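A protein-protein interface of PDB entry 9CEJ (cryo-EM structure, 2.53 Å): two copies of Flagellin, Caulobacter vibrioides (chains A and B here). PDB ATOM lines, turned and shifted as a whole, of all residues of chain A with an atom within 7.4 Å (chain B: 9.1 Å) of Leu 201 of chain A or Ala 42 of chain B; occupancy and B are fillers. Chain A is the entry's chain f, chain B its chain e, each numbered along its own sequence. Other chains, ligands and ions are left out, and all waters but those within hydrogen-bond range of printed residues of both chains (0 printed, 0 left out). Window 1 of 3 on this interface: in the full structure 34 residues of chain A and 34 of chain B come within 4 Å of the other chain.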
ATOM      1  N   ILE A  76      18.305 -16.039 -27.871  1.00  0.00           N
ATOM      2  CA  ILE A  76      18.392 -14.691 -27.320  1.00  0.00           C
ATOM      3  C   ILE A  76      19.697 -14.507 -26.554  1.00  0.00           C
ATOM      4  O   ILE A  76      20.246 -13.398 -26.512  1.00  0.00           O
ATOM      5  CB  ILE A  76      17.163 -14.356 -26.453  1.00  0.00           C
ATOM      6  CG1 ILE A  76      15.896 -14.367 -27.306  1.00  0.00           C
ATOM      7  CG2 ILE A  76      17.305 -12.990 -25.803  1.00  0.00           C
ATOM      8  CD1 ILE A  76      14.637 -14.299 -26.498  1.00  0.00           C
ATOM      9  N   ALA A  79      22.207 -13.614 -29.072  1.00  0.00           N
ATOM     10  CA  ALA A  79      21.889 -12.282 -29.582  1.00  0.00           C
ATOM     11  C   ALA A  79      22.402 -11.195 -28.643  1.00  0.00           C
ATOM     12  O   ALA A  79      23.033 -10.225 -29.080  1.00  0.00           O
ATOM     13  CB  ALA A  79      20.381 -12.150 -29.790  1.00  0.00           C
ATOM     14  N   LEU A  80      22.149 -11.345 -27.341  1.00  0.00           N
ATOM     15  CA  LEU A  80      22.672 -10.368 -26.387  1.00  0.00           C
ATOM     16  C   LEU A  80      24.192 -10.417 -26.308  1.00  0.00           C
ATOM     17  O   LEU A  80      24.831  -9.383 -26.060  1.00  0.00           O
ATOM     18  CB  LEU A  80      22.057 -10.583 -25.006  1.00  0.00           C
ATOM     19  CG  LEU A  80      20.533 -10.700 -24.963  1.00  0.00           C
ATOM     20  CD1 LEU A  80      20.071 -11.355 -23.672  1.00  0.00           C
ATOM     21  CD2 LEU A  80      19.895  -9.335 -25.144  1.00  0.00           C
ATOM     22  N   ALA A  81      24.790 -11.592 -26.526  1.00  0.00           N
ATOM     23  CA  ALA A  81      26.247 -11.669 -26.537  1.00  0.00           C
ATOM     24  C   ALA A  81      26.832 -10.835 -27.666  1.00  0.00           C
ATOM     25  O   ALA A  81      27.894 -10.222 -27.510  1.00  0.00           O
ATOM     26  CB  ALA A  81      26.696 -13.125 -26.657  1.00  0.00           C
ATOM     27  N   ALA A  82      26.144 -10.779 -28.809  1.00  0.00           N
ATOM     28  CA  ALA A  82      26.603  -9.888 -29.873  1.00  0.00           C
ATOM     29  C   ALA A  82      26.277  -8.431 -29.560  1.00  0.00           C
ATOM     30  O   ALA A  82      27.072  -7.521 -29.857  1.00  0.00           O
ATOM     31  CB  ALA A  82      25.986 -10.292 -31.208  1.00  0.00           C
ATOM     32  N   GLY A  83      25.122  -8.191 -28.939  1.00  0.00           N
ATOM     33  CA  GLY A  83      24.691  -6.826 -28.702  1.00  0.00           C
ATOM     34  C   GLY A  83      25.545  -6.099 -27.684  1.00  0.00           C
ATOM     35  O   GLY A  83      25.670  -4.872 -27.740  1.00  0.00           O
ATOM     36  N   ASP A  84      26.159  -6.835 -26.759  1.00  0.00           N
ATOM     37  CA  ASP A  84      27.038  -6.195 -25.785  1.00  0.00           C
ATOM     38  C   ASP A  84      28.250  -5.570 -26.469  1.00  0.00           C
ATOM     39  O   ASP A  84      28.582  -4.397 -26.238  1.00  0.00           O
ATOM     40  CB  ASP A  84      27.471  -7.215 -24.734  1.00  0.00           C
ATOM     41  CG  ASP A  84      26.327  -7.651 -23.844  1.00  0.00           C
ATOM     42  OD1 ASP A  84      25.395  -6.845 -23.636  1.00  0.00           O
ATOM     43  OD2 ASP A  84      26.355  -8.800 -23.356  1.00  0.00           O
ATOM     44  N   THR A  85      28.912  -6.335 -27.341  1.00  0.00           N
ATOM     45  CA  THR A  85      30.029  -5.784 -28.100  1.00  0.00           C
ATOM     46  C   THR A  85      29.572  -4.686 -29.048  1.00  0.00           C
ATOM     47  O   THR A  85      30.306  -3.710 -29.267  1.00  0.00           O
ATOM     48  CB  THR A  85      30.735  -6.889 -28.885  1.00  0.00           C
ATOM     49  OG1 THR A  85      30.978  -8.012 -28.026  1.00  0.00           O
ATOM     50  CG2 THR A  85      32.057  -6.385 -29.444  1.00  0.00           C
ATOM     51  N   ILE A  86      28.367  -4.811 -29.612  1.00  0.00           N
ATOM     52  CA  ILE A  86      27.904  -3.754 -30.508  1.00  0.00           C
ATOM     53  C   ILE A  86      27.712  -2.447 -29.747  1.00  0.00           C
ATOM     54  O   ILE A  86      28.114  -1.377 -30.219  1.00  0.00           O
ATOM     55  CB  ILE A  86      26.624  -4.179 -31.251  1.00  0.00           C
ATOM     56  CG1 ILE A  86      26.978  -5.190 -32.341  1.00  0.00           C
ATOM     57  CG2 ILE A  86      25.912  -2.971 -31.834  1.00  0.00           C
ATOM     58  CD1 ILE A  86      25.798  -5.821 -32.993  1.00  0.00           C
ATOM     59  N   THR A  87      27.119  -2.510 -28.551  1.00  0.00           N
ATOM     60  CA  THR A  87      26.973  -1.298 -27.751  1.00  0.00           C
ATOM     61  C   THR A  87      28.320  -0.745 -27.319  1.00  0.00           C
ATOM     62  O   THR A  87      28.498   0.478 -27.271  1.00  0.00           O
ATOM     63  CB  THR A  87      26.106  -1.566 -26.522  1.00  0.00           C
ATOM     64  OG1 THR A  87      26.616  -2.701 -25.811  1.00  0.00           O
ATOM     65  CG2 THR A  87      24.668  -1.821 -26.934  1.00  0.00           C
ATOM     66  N   ALA A 139      18.737 -11.334 -34.104  1.00  0.00           N
ATOM     67  CA  ALA A 139      19.355 -10.018 -34.146  1.00  0.00           C
ATOM     68  C   ALA A 139      19.897  -9.617 -35.512  1.00  0.00           C
ATOM     69  O   ALA A 139      20.247  -8.446 -35.694  1.00  0.00           O
ATOM     70  CB  ALA A 139      20.493  -9.936 -33.119  1.00  0.00           C
ATOM     71  N   LYS A 162      14.664  -7.724 -33.348  1.00  0.00           N
ATOM     72  CA  LYS A 162      15.224  -6.416 -33.030  1.00  0.00           C
ATOM     73  C   LYS A 162      16.544  -6.291 -33.775  1.00  0.00           C
ATOM     74  O   LYS A 162      17.588  -6.716 -33.268  1.00  0.00           O
ATOM     75  CB  LYS A 162      15.420  -6.249 -31.523  1.00  0.00           C
ATOM     76  CG  LYS A 162      14.139  -6.371 -30.714  1.00  0.00           C
ATOM     77  CD  LYS A 162      13.163  -5.247 -31.023  1.00  0.00           C
ATOM     78  CE  LYS A 162      11.964  -5.289 -30.086  1.00  0.00           C
ATOM     79  NZ  LYS A 162      11.092  -6.467 -30.335  1.00  0.00           N
ATOM     80  N   ILE A 164      19.964  -5.149 -35.106  1.00  0.00           N
ATOM     81  CA  ILE A 164      21.054  -4.423 -34.469  1.00  0.00           C
ATOM     82  C   ILE A 164      22.209  -4.178 -35.432  1.00  0.00           C
ATOM     83  O   ILE A 164      23.251  -3.652 -35.028  1.00  0.00           O
ATOM     84  CB  ILE A 164      21.518  -5.136 -33.189  1.00  0.00           C
ATOM     85  CG1 ILE A 164      22.050  -6.534 -33.504  1.00  0.00           C
ATOM     86  CG2 ILE A 164      20.388  -5.201 -32.170  1.00  0.00           C
ATOM     87  CD1 ILE A 164      22.723  -7.198 -32.327  1.00  0.00           C
ATOM     88  N   LEU A 194      23.001   4.531 -30.266  1.00  0.00           N
ATOM     89  CA  LEU A 194      23.233   3.829 -29.010  1.00  0.00           C
ATOM     90  C   LEU A 194      21.938   3.669 -28.231  1.00  0.00           C
ATOM     91  O   LEU A 194      21.686   2.612 -27.637  1.00  0.00           O
ATOM     92  CB  LEU A 194      24.274   4.575 -28.178  1.00  0.00           C
ATOM     93  CG  LEU A 194      24.685   3.944 -26.846  1.00  0.00           C
ATOM     94  CD1 LEU A 194      24.937   2.451 -26.993  1.00  0.00           C
ATOM     95  CD2 LEU A 194      25.909   4.642 -26.292  1.00  0.00           C
ATOM     96  N   GLN A 195      21.074   4.686 -28.276  1.00  0.00           N
ATOM     97  CA  GLN A 195      19.825   4.616 -27.526  1.00  0.00           C
ATOM     98  C   GLN A 195      18.920   3.515 -28.065  1.00  0.00           C
ATOM     99  O   GLN A 195      18.409   2.682 -27.300  1.00  0.00           O
ATOM    100  CB  GLN A 195      19.114   5.969 -27.573  1.00  0.00           C
ATOM    101  CG  GLN A 195      19.594   6.961 -26.534  1.00  0.00           C
ATOM    102  CD  GLN A 195      18.915   6.769 -25.195  1.00  0.00           C
ATOM    103  OE1 GLN A 195      18.154   5.821 -25.003  1.00  0.00           O
ATOM    104  NE2 GLN A 195      19.181   7.674 -24.261  1.00  0.00           N
ATOM    105  N   THR A 196      18.718   3.487 -29.385  1.00  0.00           N
ATOM    106  CA  THR A 196      17.858   2.452 -29.953  1.00  0.00           C
ATOM    107  C   THR A 196      18.459   1.060 -29.776  1.00  0.00           C
ATOM    108  O   THR A 196      17.716   0.089 -29.564  1.00  0.00           O
ATOM    109  CB  THR A 196      17.560   2.752 -31.428  1.00  0.00           C
ATOM    110  OG1 THR A 196      16.601   1.813 -31.929  1.00  0.00           O
ATOM    111  CG2 THR A 196      18.820   2.708 -32.279  1.00  0.00           C
ATOM    112  N   ALA A 197      19.792   0.945 -29.789  1.00  0.00           N
ATOM    113  CA  ALA A 197      20.413  -0.359 -29.580  1.00  0.00           C
ATOM    114  C   ALA A 197      20.165  -0.871 -28.166  1.00  0.00           C
ATOM    115  O   ALA A 197      19.791  -2.038 -27.973  1.00  0.00           O
ATOM    116  CB  ALA A 197      21.912  -0.275 -29.871  1.00  0.00           C
ATOM    117  N   THR A 198      20.366  -0.013 -27.159  1.00  0.00           N
ATOM    118  CA  THR A 198      20.111  -0.447 -25.787  1.00  0.00           C
ATOM    119  C   THR A 198      18.637  -0.757 -25.558  1.00  0.00           C
ATOM    120  O   THR A 198      18.304  -1.694 -24.821  1.00  0.00           O
ATOM    121  CB  THR A 198      20.598   0.600 -24.782  1.00  0.00           C
ATOM    122  OG1 THR A 198      19.694   1.710 -24.762  1.00  0.00           O
ATOM    123  CG2 THR A 198      22.013   1.055 -25.092  1.00  0.00           C
ATOM    124  N   ASN A 199      17.734  -0.009 -26.200  1.00  0.00           N
ATOM    125  CA  ASN A 199      16.315  -0.312 -26.017  1.00  0.00           C
ATOM    126  C   ASN A 199      15.964  -1.669 -26.617  1.00  0.00           C
ATOM    127  O   ASN A 199      15.211  -2.454 -26.014  1.00  0.00           O
ATOM    128  CB  ASN A 199      15.456   0.791 -26.634  1.00  0.00           C
ATOM    129  CG  ASN A 199      15.574   2.107 -25.891  1.00  0.00           C
ATOM    130  OD1 ASN A 199      15.642   2.136 -24.662  1.00  0.00           O
ATOM    131  ND2 ASN A 199      15.592   3.206 -26.634  1.00  0.00           N
ATOM    132  N   LYS A 200      16.539  -1.984 -27.781  1.00  0.00           N
ATOM    133  CA  LYS A 200      16.272  -3.275 -28.405  1.00  0.00           C
ATOM    134  C   LYS A 200      16.810  -4.414 -27.547  1.00  0.00           C
ATOM    135  O   LYS A 200      16.136  -5.434 -27.343  1.00  0.00           O
ATOM    136  CB  LYS A 200      16.895  -3.308 -29.801  1.00  0.00           C
ATOM    137  CG  LYS A 200      16.010  -2.720 -30.887  1.00  0.00           C
ATOM    138  CD  LYS A 200      16.835  -2.294 -32.089  1.00  0.00           C
ATOM    139  CE  LYS A 200      15.954  -1.884 -33.253  1.00  0.00           C
ATOM    140  NZ  LYS A 200      16.716  -1.095 -34.255  1.00  0.00           N
ATOM    141  N   LEU A 201      18.026  -4.247 -27.019  1.00  0.00           N
ATOM    142  CA  LEU A 201      18.596  -5.291 -26.174  1.00  0.00           C
ATOM    143  C   LEU A 201      17.799  -5.474 -24.886  1.00  0.00           C
ATOM    144  O   LEU A 201      17.650  -6.607 -24.403  1.00  0.00           O
ATOM    145  CB  LEU A 201      20.058  -4.969 -25.867  1.00  0.00           C
ATOM    146  CG  LEU A 201      20.982  -4.997 -27.088  1.00  0.00           C
ATOM    147  CD1 LEU A 201      22.380  -4.535 -26.730  1.00  0.00           C
ATOM    148  CD2 LEU A 201      21.016  -6.377 -27.722  1.00  0.00           C
ATOM    149  N   ALA A 202      17.253  -4.386 -24.334  1.00  0.00           N
ATOM    150  CA  ALA A 202      16.437  -4.509 -23.130  1.00  0.00           C
ATOM    151  C   ALA A 202      15.156  -5.286 -23.407  1.00  0.00           C
ATOM    152  O   ALA A 202      14.751  -6.142 -22.603  1.00  0.00           O
ATOM    153  CB  ALA A 202      16.115  -3.122 -22.575  1.00  0.00           C
ATOM    154  N   SER A 203      14.512  -5.016 -24.546  1.00  0.00           N
ATOM    155  CA  SER A 203      13.324  -5.793 -24.887  1.00  0.00           C
ATOM    156  C   SER A 203      13.661  -7.263 -25.114  1.00  0.00           C
ATOM    157  O   SER A 203      12.886  -8.151 -24.724  1.00  0.00           O
ATOM    158  CB  SER A 203      12.644  -5.206 -26.123  1.00  0.00           C
ATOM    159  OG  SER A 203      11.340  -5.733 -26.284  1.00  0.00           O
ATOM    160  N   LEU A 204      14.830  -7.541 -25.702  1.00  0.00           N
ATOM    161  CA  LEU A 204      15.238  -8.930 -25.906  1.00  0.00           C
ATOM    162  C   LEU A 204      15.430  -9.648 -24.575  1.00  0.00           C
ATOM    163  O   LEU A 204      15.010 -10.802 -24.404  1.00  0.00           O
ATOM    164  CB  LEU A 204      16.524  -8.981 -26.730  1.00  0.00           C
ATOM    165  CG  LEU A 204      16.439  -8.650 -28.220  1.00  0.00           C
ATOM    166  CD1 LEU A 204      17.816  -8.729 -28.856  1.00  0.00           C
ATOM    167  CD2 LEU A 204      15.478  -9.593 -28.919  1.00  0.00           C
ATOM    168  N   GLY A 205      16.036  -8.967 -23.602  1.00  0.00           N
ATOM    169  CA  GLY A 205      16.257  -9.604 -22.316  1.00  0.00           C
ATOM    170  C   GLY A 205      14.966  -9.843 -21.558  1.00  0.00           C
ATOM    171  O   GLY A 205      14.795 -10.882 -20.908  1.00  0.00           O
ATOM    172  N   THR A 206      14.019  -8.904 -21.661  1.00  0.00           N
ATOM    173  CA  THR A 206      12.728  -9.119 -21.015  1.00  0.00           C
ATOM    174  C   THR A 206      11.991 -10.298 -21.640  1.00  0.00           C
ATOM    175  O   THR A 206      11.386 -11.116 -20.926  1.00  0.00           O
ATOM    176  CB  THR A 206      11.882  -7.849 -21.099  1.00  0.00           C
ATOM    177  OG1 THR A 206      12.609  -6.753 -20.530  1.00  0.00           O
ATOM    178  CG2 THR A 206      10.573  -8.028 -20.347  1.00  0.00           C
ATOM    179  N   SER A 207      12.065 -10.428 -22.968  1.00  0.00           N
ATOM    180  CA  SER A 207      11.429 -11.570 -23.613  1.00  0.00           C
ATOM    181  C   SER A 207      12.078 -12.882 -23.194  1.00  0.00           C
ATOM    182  O   SER A 207      11.382 -13.888 -23.008  1.00  0.00           O
ATOM    183  CB  SER A 207      11.482 -11.405 -25.131  1.00  0.00           C
ATOM    184  OG  SER A 207      12.818 -11.455 -25.597  1.00  0.00           O
ATOM    185  N   SER A 208      13.400 -12.888 -23.000  1.00  0.00           N
ATOM    186  CA  SER A 208      14.064 -14.112 -22.556  1.00  0.00           C
ATOM    187  C   SER A 208      13.650 -14.496 -21.137  1.00  0.00           C
ATOM    188  O   SER A 208      13.466 -15.686 -20.829  1.00  0.00           O
ATOM    189  CB  SER A 208      15.578 -13.941 -22.638  1.00  0.00           C
ATOM    190  OG  SER A 208      16.061 -13.199 -21.538  1.00  0.00           O
ATOM    191  N   VAL A 209      13.501 -13.503 -20.254  1.00  0.00           N
ATOM    192  CA  VAL A 209      13.067 -13.809 -18.892  1.00  0.00           C
ATOM    193  C   VAL A 209      11.650 -14.370 -18.898  1.00  0.00           C
ATOM    194  O   VAL A 209      11.332 -15.319 -18.161  1.00  0.00           O
ATOM    195  CB  VAL A 209      13.182 -12.560 -18.001  1.00  0.00           C
ATOM    196  CG1 VAL A 209      12.704 -12.868 -16.596  1.00  0.00           C
ATOM    197  CG2 VAL A 209      14.613 -12.075 -17.967  1.00  0.00           C
ATOM    198  N   LYS B  38      24.569  -6.394  -9.526  1.00  0.00           N
ATOM    199  CA  LYS B  38      23.225  -6.948  -9.457  1.00  0.00           C
ATOM    200  C   LYS B  38      22.451  -6.775 -10.757  1.00  0.00           C
ATOM    201  O   LYS B  38      21.378  -7.368 -10.904  1.00  0.00           O
ATOM    202  CB  LYS B  38      22.442  -6.321  -8.298  1.00  0.00           C
ATOM    203  CG  LYS B  38      22.185  -4.837  -8.434  1.00  0.00           C
ATOM    204  CD  LYS B  38      21.460  -4.298  -7.215  1.00  0.00           C
ATOM    205  CE  LYS B  38      21.177  -2.816  -7.359  1.00  0.00           C
ATOM    206  NZ  LYS B  38      22.428  -2.014  -7.348  1.00  0.00           N
ATOM    207  N   ILE B  39      22.967  -5.983 -11.697  1.00  0.00           N
ATOM    208  CA  ILE B  39      22.380  -5.860 -13.026  1.00  0.00           C
ATOM    209  C   ILE B  39      23.526  -5.931 -14.031  1.00  0.00           C
ATOM    210  O   ILE B  39      23.951  -4.914 -14.589  1.00  0.00           O
ATOM    211  CB  ILE B  39      21.559  -4.563 -13.169  1.00  0.00           C
ATOM    212  CG1 ILE B  39      20.381  -4.572 -12.194  1.00  0.00           C
ATOM    213  CG2 ILE B  39      20.994  -4.426 -14.573  1.00  0.00           C
ATOM    214  CD1 ILE B  39      19.674  -3.246 -12.075  1.00  0.00           C
ATOM    215  N   ALA B  40      24.067  -7.134 -14.227  1.00  0.00           N
ATOM    216  CA  ALA B  40      25.189  -7.321 -15.137  1.00  0.00           C
ATOM    217  C   ALA B  40      24.792  -7.217 -16.604  1.00  0.00           C
ATOM    218  O   ALA B  40      25.661  -6.977 -17.450  1.00  0.00           O
ATOM    219  CB  ALA B  40      25.851  -8.675 -14.883  1.00  0.00           C
ATOM    220  N   SER B  41      23.514  -7.394 -16.925  1.00  0.00           N
ATOM    221  CA  SER B  41      23.081  -7.440 -18.315  1.00  0.00           C
ATOM    222  C   SER B  41      21.594  -7.129 -18.380  1.00  0.00           C
ATOM    223  O   SER B  41      20.920  -6.994 -17.358  1.00  0.00           O
ATOM    224  CB  SER B  41      23.386  -8.803 -18.945  1.00  0.00           C
ATOM    225  OG  SER B  41      22.452  -9.779 -18.520  1.00  0.00           O
ATOM    226  N   ALA B  42      21.091  -7.018 -19.611  1.00  0.00           N
ATOM    227  CA  ALA B  42      19.667  -6.807 -19.840  1.00  0.00           C
ATOM    228  C   ALA B  42      18.818  -7.966 -19.343  1.00  0.00           C
ATOM    229  O   ALA B  42      17.615  -7.784 -19.137  1.00  0.00           O
ATOM    230  CB  ALA B  42      19.400  -6.574 -21.328  1.00  0.00           C
ATOM    231  N   LYS B  43      19.409  -9.150 -19.174  1.00  0.00           N
ATOM    232  CA  LYS B  43      18.699 -10.283 -18.596  1.00  0.00           C
ATOM    233  C   LYS B  43      18.236 -10.010 -17.169  1.00  0.00           C
ATOM    234  O   LYS B  43      17.219 -10.567 -16.745  1.00  0.00           O
ATOM    235  CB  LYS B  43      19.608 -11.516 -18.628  1.00  0.00           C
ATOM    236  CG  LYS B  43      18.997 -12.805 -18.102  1.00  0.00           C
ATOM    237  CD  LYS B  43      17.879 -13.308 -18.990  1.00  0.00           C
ATOM    238  CE  LYS B  43      17.273 -14.591 -18.439  1.00  0.00           C
ATOM    239  NZ  LYS B  43      18.231 -15.731 -18.468  1.00  0.00           N
ATOM    240  N   ASP B  44      18.949  -9.165 -16.424  1.00  0.00           N
ATOM    241  CA  ASP B  44      18.586  -8.871 -15.042  1.00  0.00           C
ATOM    242  C   ASP B  44      17.505  -7.801 -14.929  1.00  0.00           C
ATOM    243  O   ASP B  44      16.577  -7.942 -14.125  1.00  0.00           O
ATOM    244  CB  ASP B  44      19.827  -8.431 -14.262  1.00  0.00           C
ATOM    245  CG  ASP B  44      20.889  -9.513 -14.194  1.00  0.00           C
ATOM    246  OD1 ASP B  44      22.085  -9.165 -14.107  1.00  0.00           O
ATOM    247  OD2 ASP B  44      20.529 -10.708 -14.230  1.00  0.00           O
ATOM    248  N   ASN B  45      17.600  -6.744 -15.737  1.00  0.00           N
ATOM    249  CA  ASN B  45      16.690  -5.605 -15.673  1.00  0.00           C
ATOM    250  C   ASN B  45      16.983  -4.676 -16.845  1.00  0.00           C
ATOM    251  O   ASN B  45      17.961  -3.922 -16.811  1.00  0.00           O
ATOM    252  CB  ASN B  45      16.846  -4.863 -14.342  1.00  0.00           C
ATOM    253  CG  ASN B  45      15.783  -3.799 -14.133  1.00  0.00           C
ATOM    254  OD1 ASN B  45      14.928  -3.576 -14.986  1.00  0.00           O
ATOM    255  ND2 ASN B  45      15.835  -3.136 -12.985  1.00  0.00           N
ATOM    256  N   GLY B  46      16.139  -4.717 -17.879  1.00  0.00           N
ATOM    257  CA  GLY B  46      16.502  -4.085 -19.138  1.00  0.00           C
ATOM    258  C   GLY B  46      16.541  -2.568 -19.088  1.00  0.00           C
ATOM    259  O   GLY B  46      17.402  -1.944 -19.714  1.00  0.00           O
ATOM    260  N   ALA B  47      15.626  -1.952 -18.334  1.00  0.00           N
ATOM    261  CA  ALA B  47      15.537  -0.494 -18.339  1.00  0.00           C
ATOM    262  C   ALA B  47      16.685   0.146 -17.570  1.00  0.00           C
ATOM    263  O   ALA B  47      17.335   1.075 -18.070  1.00  0.00           O
ATOM    264  CB  ALA B  47      14.195  -0.050 -17.759  1.00  0.00           C
ATOM    265  N   ILE B  48      16.952  -0.334 -16.354  1.00  0.00           N
ATOM    266  CA  ILE B  48      18.067   0.211 -15.586  1.00  0.00           C
ATOM    267  C   ILE B  48      19.385  -0.094 -16.283  1.00  0.00           C
ATOM    268  O   ILE B  48      20.309   0.725 -16.275  1.00  0.00           O
ATOM    269  CB  ILE B  48      18.046  -0.333 -14.146  1.00  0.00           C
ATOM    270  CG1 ILE B  48      16.732   0.031 -13.458  1.00  0.00           C
ATOM    271  CG2 ILE B  48      19.223   0.212 -13.350  1.00  0.00           C
ATOM    272  CD1 ILE B  48      16.495   1.518 -13.339  1.00  0.00           C
ATOM    273  N   TRP B  49      19.478  -1.258 -16.933  1.00  0.00           N
ATOM    274  CA  TRP B  49      20.704  -1.600 -17.646  1.00  0.00           C
ATOM    275  C   TRP B  49      20.910  -0.697 -18.855  1.00  0.00           C
ATOM    276  O   TRP B  49      22.034  -0.265 -19.129  1.00  0.00           O
ATOM    277  CB  TRP B  49      20.678  -3.069 -18.068  1.00  0.00           C
ATOM    278  CG  TRP B  49      21.722  -3.431 -19.083  1.00  0.00           C
ATOM    279  CD1 TRP B  49      22.983  -3.883 -18.827  1.00  0.00           C
ATOM    280  CD2 TRP B  49      21.595  -3.390 -20.509  1.00  0.00           C
ATOM    281  NE1 TRP B  49      23.652  -4.114 -20.002  1.00  0.00           N
ATOM    282  CE2 TRP B  49      22.822  -3.819 -21.050  1.00  0.00           C
ATOM    283  CE3 TRP B  49      20.566  -3.024 -21.382  1.00  0.00           C
ATOM    284  CZ2 TRP B  49      23.047  -3.893 -22.421  1.00  0.00           C
ATOM    285  CZ3 TRP B  49      20.793  -3.099 -22.743  1.00  0.00           C
ATOM    286  CH2 TRP B  49      22.023  -3.530 -23.249  1.00  0.00           C
ATOM    287  N   ALA B  50      19.833  -0.377 -19.578  1.00  0.00           N
ATOM    288  CA  ALA B  50      19.959   0.520 -20.722  1.00  0.00           C
ATOM    289  C   ALA B  50      20.347   1.922 -20.274  1.00  0.00           C
ATOM    290  O   ALA B  50      21.218   2.566 -20.880  1.00  0.00           O
ATOM    291  CB  ALA B  50      18.651   0.546 -21.513  1.00  0.00           C
ATOM    292  N   LYS B  53      23.913   1.898 -19.572  1.00  0.00           N
ATOM    293  CA  LYS B  53      24.750   1.888 -20.769  1.00  0.00           C
ATOM    294  C   LYS B  53      24.919   3.293 -21.330  1.00  0.00           C
ATOM    295  O   LYS B  53      26.045   3.733 -21.616  1.00  0.00           O
ATOM    296  CB  LYS B  53      24.158   0.960 -21.831  1.00  0.00           C
ATOM    297  CG  LYS B  53      24.082  -0.496 -21.424  1.00  0.00           C
ATOM    298  CD  LYS B  53      25.466  -1.078 -21.208  1.00  0.00           C
ATOM    299  CE  LYS B  53      26.205  -1.236 -22.523  1.00  0.00           C
ATOM    300  NZ  LYS B  53      27.534  -1.876 -22.330  1.00  0.00           N
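O of Gly 205 of chain A sits at hydrogen-bond distance from OG of Ser 208 of chain A (2.7 Å).
The backbone carbonyl oxygen (O) of Gly 83 of chain A sits at hydrogen-bond distance from the side-chain hydroxyl (OG1) of Thr 87 of chain A.
The side-chain hydroxyl (OG) of Ser 41 of chain B sits close to the backbone NH (N) of Lys 43 of chain B (3.2 Å).
O of Asp 84 of chain A sits at hydrogen-bond distance from OG1 of Thr 87 of chain A, at 2.6 Å.
OG1 of Thr 206 of chain A sits at hydrogen-bond distance from O of Ala 202 of chain A (3.0 Å).
The side-chain hydroxyl of Thr 198 of chain A is in hydrogen-bond range of the backbone carbonyl oxygen of Gln 195 of chain A, at 3.0 Å.
Among the printed residues, merely in contact across the chains: Ser 208 of chain A with Lys 43 of chain B (3.1 Å), Val 209 of chain A with Lys 43 of chain B (3.2 Å), Ala 202 of chain A with Gly 46 of chain B (3.4 Å), Thr 198 of chain A with Trp 49 of chain B (3.5 Å), Leu 201 of chain A with Ala 42 of chain B (3.5 Å), Leu 201 of chain A with Trp 49 of chain B (3.6 Å), Thr 198 of chain A with Ala 50 of chain B (3.6 Å), Thr 87 of chain A with Lys 53 of chain B (3.6 Å), Thr 198 of chain A with Lys 53 of chain B (3.9 Å), Gly 205 of chain A with Ala 42 of chain B (3.9 Å) and Asp 84 of chain A with Trp 49 of chain B (3.96 Å).
No residue of chain B comes within 4 Å of Gly 83 of chain A.
Of the printed residues of chain B, Thr 87 of chain A touches Lys 53.
Ile 164 of chain A touches none of the printed residues of chain B.
Of the printed residues of chain B, Thr 198 of chain A touches Trp 49 (3.5 Å), Ala 50 (3.6 Å) and Lys 53 (3.9 Å).
Printed residues of chain B within 4 Å of Ala 202 of chain A: Gly 46 (3.4 Å).
The nearest residue of chain B that does not touch Leu 201 of chain A is Gly 46 of chain B (5.9 Å).
The nearest residue of chain A that does not touch Ala 42 of chain B is Ala 202 of chain A (4.04 Å).
Hydrophobic or aromatic side chains of chain A that line the printed part of chain B: Leu 201, Ala 202 and Val 209.
Of the 14 printed residues of chain B, 6 touch a printed residue of chain A.
Printed residues of chain B that touch a printed residue of chain A: Ala 42, Lys 43, Gly 46, Trp 49, Ala 50 and Lys 53.
Among the printed residues, 11 pairs touch across the chains.
No position is printed for both chains.
Of the 11 pairs that touch across the chains among the printed residues, none has its exchanged pair printed and touching as well.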
